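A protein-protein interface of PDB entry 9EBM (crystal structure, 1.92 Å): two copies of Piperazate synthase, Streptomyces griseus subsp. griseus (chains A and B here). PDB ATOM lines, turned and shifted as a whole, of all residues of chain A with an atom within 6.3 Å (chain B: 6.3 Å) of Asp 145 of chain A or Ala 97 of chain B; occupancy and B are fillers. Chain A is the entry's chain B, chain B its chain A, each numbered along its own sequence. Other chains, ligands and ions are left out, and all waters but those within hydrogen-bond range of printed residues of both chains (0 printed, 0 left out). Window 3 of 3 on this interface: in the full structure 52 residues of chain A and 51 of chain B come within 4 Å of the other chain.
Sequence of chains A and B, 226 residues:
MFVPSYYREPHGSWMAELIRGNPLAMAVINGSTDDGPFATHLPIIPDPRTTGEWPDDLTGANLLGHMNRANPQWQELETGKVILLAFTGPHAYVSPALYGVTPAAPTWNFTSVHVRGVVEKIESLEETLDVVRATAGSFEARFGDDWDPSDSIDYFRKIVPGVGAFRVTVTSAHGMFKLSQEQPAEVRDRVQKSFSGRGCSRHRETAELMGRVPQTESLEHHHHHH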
ATOM      1  N   GLU A 140      19.040  13.003   1.378  1.00  0.00           N
ATOM      2  CA  GLU A 140      19.086  14.232   0.589  1.00  0.00           C
ATOM      3  C   GLU A 140      17.710  14.879   0.505  1.00  0.00           C
ATOM      4  O   GLU A 140      17.584  16.104   0.593  1.00  0.00           O
ATOM      5  CB  GLU A 140      19.641  13.944  -0.811  1.00  0.00           C
ATOM      6  CG  GLU A 140      19.753  15.179  -1.726  1.00  0.00           C
ATOM      7  CD  GLU A 140      20.740  16.224  -1.222  1.00  0.00           C
ATOM      8  OE1 GLU A 140      21.617  15.889  -0.391  1.00  0.00           O
ATOM      9  OE2 GLU A 140      20.632  17.392  -1.662  1.00  0.00           O
ATOM     10  N   ALA A 141      16.663  14.073   0.355  1.00  0.00           N
ATOM     11  CA  ALA A 141      15.315  14.628   0.328  1.00  0.00           C
ATOM     12  C   ALA A 141      14.951  15.250   1.668  1.00  0.00           C
ATOM     13  O   ALA A 141      14.333  16.318   1.717  1.00  0.00           O
ATOM     14  CB  ALA A 141      14.312  13.538  -0.048  1.00  0.00           C
ATOM     15  N   PHE A 143      17.025  16.192   4.376  1.00  0.00           N
ATOM     16  CA  PHE A 143      17.941  17.160   4.967  1.00  0.00           C
ATOM     17  C   PHE A 143      18.703  17.996   3.950  1.00  0.00           C
ATOM     18  O   PHE A 143      19.457  18.886   4.352  1.00  0.00           O
ATOM     19  CB  PHE A 143      18.981  16.455   5.851  1.00  0.00           C
ATOM     20  CG  PHE A 143      18.408  15.441   6.816  1.00  0.00           C
ATOM     21  CD1 PHE A 143      17.718  15.846   7.947  1.00  0.00           C
ATOM     22  CD2 PHE A 143      18.610  14.081   6.615  1.00  0.00           C
ATOM     23  CE1 PHE A 143      17.215  14.910   8.844  1.00  0.00           C
ATOM     24  CE2 PHE A 143      18.110  13.146   7.509  1.00  0.00           C
ATOM     25  CZ  PHE A 143      17.409  13.565   8.623  1.00  0.00           C
ATOM     26  N   GLY A 144      18.560  17.725   2.658  1.00  0.00           N
ATOM     27  CA  GLY A 144      19.465  18.302   1.685  1.00  0.00           C
ATOM     28  C   GLY A 144      18.904  19.431   0.850  1.00  0.00           C
ATOM     29  O   GLY A 144      18.180  20.296   1.352  1.00  0.00           O
ATOM     30  N   ASP A 145      19.232  19.418  -0.442  1.00  0.00           N
ATOM     31  CA  ASP A 145      19.006  20.566  -1.305  1.00  0.00           C
ATOM     32  C   ASP A 145      18.913  20.143  -2.772  1.00  0.00           C
ATOM     33  O   ASP A 145      19.550  20.743  -3.641  1.00  0.00           O
ATOM     34  CB  ASP A 145      20.135  21.581  -1.090  1.00  0.00           C
ATOM     35  CG  ASP A 145      19.801  22.959  -1.620  1.00  0.00           C
ATOM     36  OD1 ASP A 145      18.653  23.165  -2.076  1.00  0.00           O
ATOM     37  OD2 ASP A 145      20.696  23.835  -1.581  1.00  0.00           O
ATOM     38  N   ASP A 146      18.141  19.089  -3.049  1.00  0.00           N
ATOM     39  CA  ASP A 146      17.813  18.676  -4.419  1.00  0.00           C
ATOM     40  C   ASP A 146      19.055  18.319  -5.236  1.00  0.00           C
ATOM     41  O   ASP A 146      19.192  18.710  -6.397  1.00  0.00           O
ATOM     42  CB  ASP A 146      16.994  19.754  -5.129  1.00  0.00           C
ATOM     43  CG  ASP A 146      15.642  19.961  -4.493  1.00  0.00           C
ATOM     44  OD1 ASP A 146      14.893  18.969  -4.371  1.00  0.00           O
ATOM     45  OD2 ASP A 146      15.335  21.112  -4.108  1.00  0.00           O
ATOM     46  N   TRP A 147      19.965  17.562  -4.639  1.00  0.00           N
ATOM     47  CA  TRP A 147      21.139  17.123  -5.373  1.00  0.00           C
ATOM     48  C   TRP A 147      20.802  15.905  -6.220  1.00  0.00           C
ATOM     49  O   TRP A 147      20.120  14.983  -5.764  1.00  0.00           O
ATOM     50  CB  TRP A 147      22.279  16.797  -4.412  1.00  0.00           C
ATOM     51  CG  TRP A 147      23.452  16.202  -5.100  1.00  0.00           C
ATOM     52  CD1 TRP A 147      24.285  16.817  -5.995  1.00  0.00           C
ATOM     53  CD2 TRP A 147      23.926  14.866  -4.960  1.00  0.00           C
ATOM     54  NE1 TRP A 147      25.259  15.940  -6.411  1.00  0.00           N
ATOM     55  CE2 TRP A 147      25.059  14.733  -5.792  1.00  0.00           C
ATOM     56  CE3 TRP A 147      23.509  13.768  -4.207  1.00  0.00           C
ATOM     57  CZ2 TRP A 147      25.776  13.542  -5.890  1.00  0.00           C
ATOM     58  CZ3 TRP A 147      24.217  12.587  -4.309  1.00  0.00           C
ATOM     59  CH2 TRP A 147      25.343  12.484  -5.133  1.00  0.00           C
ATOM     60  N   TYR B  93      24.163  16.910   8.421  1.00  0.00           N
ATOM     61  CA  TYR B  93      24.141  16.298   7.105  1.00  0.00           C
ATOM     62  C   TYR B  93      24.786  17.227   6.084  1.00  0.00           C
ATOM     63  O   TYR B  93      24.530  18.434   6.074  1.00  0.00           O
ATOM     64  CB  TYR B  93      22.710  15.991   6.687  1.00  0.00           C
ATOM     65  CG  TYR B  93      22.613  15.501   5.252  1.00  0.00           C
ATOM     66  CD1 TYR B  93      22.990  14.206   4.915  1.00  0.00           C
ATOM     67  CD2 TYR B  93      22.160  16.336   4.238  1.00  0.00           C
ATOM     68  CE1 TYR B  93      22.902  13.748   3.585  1.00  0.00           C
ATOM     69  CE2 TYR B  93      22.065  15.891   2.921  1.00  0.00           C
ATOM     70  CZ  TYR B  93      22.440  14.599   2.602  1.00  0.00           C
ATOM     71  OH  TYR B  93      22.338  14.170   1.290  1.00  0.00           O
ATOM     72  N   VAL B  94      25.604  16.653   5.203  1.00  0.00           N
ATOM     73  CA  VAL B  94      26.294  17.400   4.152  1.00  0.00           C
ATOM     74  C   VAL B  94      25.706  16.996   2.808  1.00  0.00           C
ATOM     75  O   VAL B  94      25.947  15.879   2.332  1.00  0.00           O
ATOM     76  CB  VAL B  94      27.806  17.144   4.166  1.00  0.00           C
ATOM     77  CG1 VAL B  94      28.476  17.937   3.055  1.00  0.00           C
ATOM     78  CG2 VAL B  94      28.407  17.469   5.549  1.00  0.00           C
ATOM     79  N   SER B  95      24.966  17.912   2.178  1.00  0.00           N
ATOM     80  CA  SER B  95      24.440  17.670   0.838  1.00  0.00           C
ATOM     81  C   SER B  95      25.502  17.995  -0.205  1.00  0.00           C
ATOM     82  O   SER B  95      26.118  19.067  -0.135  1.00  0.00           O
ATOM     83  CB  SER B  95      23.211  18.522   0.575  1.00  0.00           C
ATOM     84  OG  SER B  95      23.036  18.687  -0.828  1.00  0.00           O
ATOM     85  N   PRO B  96      25.725  17.123  -1.198  1.00  0.00           N
ATOM     86  CA  PRO B  96      26.717  17.436  -2.238  1.00  0.00           C
ATOM     87  C   PRO B  96      26.373  18.671  -3.052  1.00  0.00           C
ATOM     88  O   PRO B  96      27.234  19.156  -3.800  1.00  0.00           O
ATOM     89  CB  PRO B  96      26.731  16.173  -3.115  1.00  0.00           C
ATOM     90  CG  PRO B  96      26.190  15.089  -2.239  1.00  0.00           C
ATOM     91  CD  PRO B  96      25.195  15.753  -1.328  1.00  0.00           C
ATOM     92  N   ALA B  97      25.146  19.190  -2.937  1.00  0.00           N
ATOM     93  CA  ALA B  97      24.808  20.424  -3.634  1.00  0.00           C
ATOM     94  C   ALA B  97      25.699  21.571  -3.185  1.00  0.00           C
ATOM     95  O   ALA B  97      25.920  22.522  -3.943  1.00  0.00           O
ATOM     96  CB  ALA B  97      23.339  20.777  -3.405  1.00  0.00           C
ATOM     97  N   LEU B  98      26.214  21.497  -1.956  1.00  0.00           N
ATOM     98  CA  LEU B  98      27.122  22.516  -1.453  1.00  0.00           C
ATOM     99  C   LEU B  98      28.493  22.427  -2.102  1.00  0.00           C
ATOM    100  O   LEU B  98      29.202  23.435  -2.148  1.00  0.00           O
ATOM    101  CB  LEU B  98      27.261  22.394   0.070  1.00  0.00           C
ATOM    102  CG  LEU B  98      25.968  22.251   0.870  1.00  0.00           C
ATOM    103  CD1 LEU B  98      26.282  22.026   2.338  1.00  0.00           C
ATOM    104  CD2 LEU B  98      25.091  23.480   0.692  1.00  0.00           C
ATOM    105  N   TYR B  99      28.868  21.251  -2.623  1.00  0.00           N
ATOM    106  CA  TYR B  99      30.235  21.032  -3.095  1.00  0.00           C
ATOM    107  C   TYR B  99      30.529  21.818  -4.362  1.00  0.00           C
ATOM    108  O   TYR B  99      31.629  22.364  -4.518  1.00  0.00           O
ATOM    109  CB  TYR B  99      30.478  19.549  -3.369  1.00  0.00           C
ATOM    110  CG  TYR B  99      30.514  18.640  -2.161  1.00  0.00           C
ATOM    111  CD1 TYR B  99      30.560  19.147  -0.862  1.00  0.00           C
ATOM    112  CD2 TYR B  99      30.503  17.264  -2.326  1.00  0.00           C
ATOM    113  CE1 TYR B  99      30.602  18.292   0.236  1.00  0.00           C
ATOM    114  CE2 TYR B  99      30.531  16.413  -1.249  1.00  0.00           C
ATOM    115  CZ  TYR B  99      30.586  16.927   0.033  1.00  0.00           C
ATOM    116  OH  TYR B  99      30.622  16.048   1.092  1.00  0.00           O
ATOM    117  N   GLY B 100      29.578  21.853  -5.292  1.00  0.00           N
ATOM    118  CA  GLY B 100      29.859  22.364  -6.614  1.00  0.00           C
ATOM    119  C   GLY B 100      30.814  21.517  -7.420  1.00  0.00           C
ATOM    120  O   GLY B 100      31.428  22.026  -8.361  1.00  0.00           O
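The backbone NH of Asp 145 of chain A sits at hydrogen-bond distance from the side-chain carboxylate of Glu 140 of chain A (2.7 Å).
The backbone NH (N) of Asp 146 of chain A sits at hydrogen-bond distance from the side-chain carboxylate (OE2) of Glu 140 of chain A (3.3 Å).
OG of Ser 95 of chain B sits close to N of Ala 97 of chain B (3.0 Å).
The side-chain carboxylate (OE2) of Glu 140 of chain A sits at hydrogen-bond distance from the backbone NH (N) of Trp 147 of chain A.
Pro 96 of chain B touches Glu 140 of chain A.
CD2 of Tyr 93 of chain B touches CB of Phe 143 of chain A, 3.6 Å away.
Gly 144 of chain A touches Tyr 93 of chain B.
Gly 144 of chain A touches Ser 95 of chain B (CA to CB, 3.9 Å).
Ser 95 of chain B touches Asp 145 of chain A.
Asp 145 of chain A touches Ala 97 of chain B.
Trp 147 of chain A touches Pro 96 of chain B (CE2 to CB, 3.5 Å).
N of Ala 97 of chain B touches CD1 of Trp 147 of chain A, at 3.97 Å.
The side-chain carboxylate (OE1) of Glu 140 of chain A is in hydrogen-bond range of the side-chain hydroxyl (OH) of Tyr 93 of chain B (2.5 Å).
The side-chain carboxylate of Glu 140 of chain A is in hydrogen-bond range of the side-chain hydroxyl of Ser 95 of chain B.
Of the 7 printed residues of chain A, 5 touch a printed residue of chain B.
Printed residues of chain B that touch a printed residue of chain A: Tyr 93, Ser 95, Pro 96 and Ala 97.
Hydrophobic or aromatic side chains of chain B within 4 Å of the printed part of chain A: Tyr 93, Pro 96 and Ala 97.
Among the printed residues, no Asp or Glu carboxylate lies within 4 Å of a Lys or Arg side-chain nitrogen of the other chain.
No position is printed for both chains.
Of chain B, only Ser 95 and Ala 97 come within 4 Å of Asp 145 of chain A.
Ala 97 of chain B touches just these residues of chain A: Asp 145 (3.8 Å) and Trp 147 (3.97 Å).
Of the printed residues of chain A, Ser 95 of chain B touches Glu 140 (2.9 Å), Gly 144 (3.9 Å) and Asp 145 (3.9 Å).
Of the printed residues of chain B, Gly 144 of chain A touches Tyr 93 (3.8 Å) and Ser 95 (3.9 Å).
Printed residues of chain B within 4 Å of Phe 143 of chain A: Tyr 93 (3.6 Å).
Of the printed residues of chain B, Glu 140 of chain A touches Tyr 93 (2.5 Å), Ser 95 (2.9 Å) and Pro 96 (3.7 Å).
Tyr 99 of chain B touches none of the printed residues of chain A.
The nearest printed residue of chain A that does not touch Tyr 93 of chain B is Trp 147 of chain A (5.6 Å).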
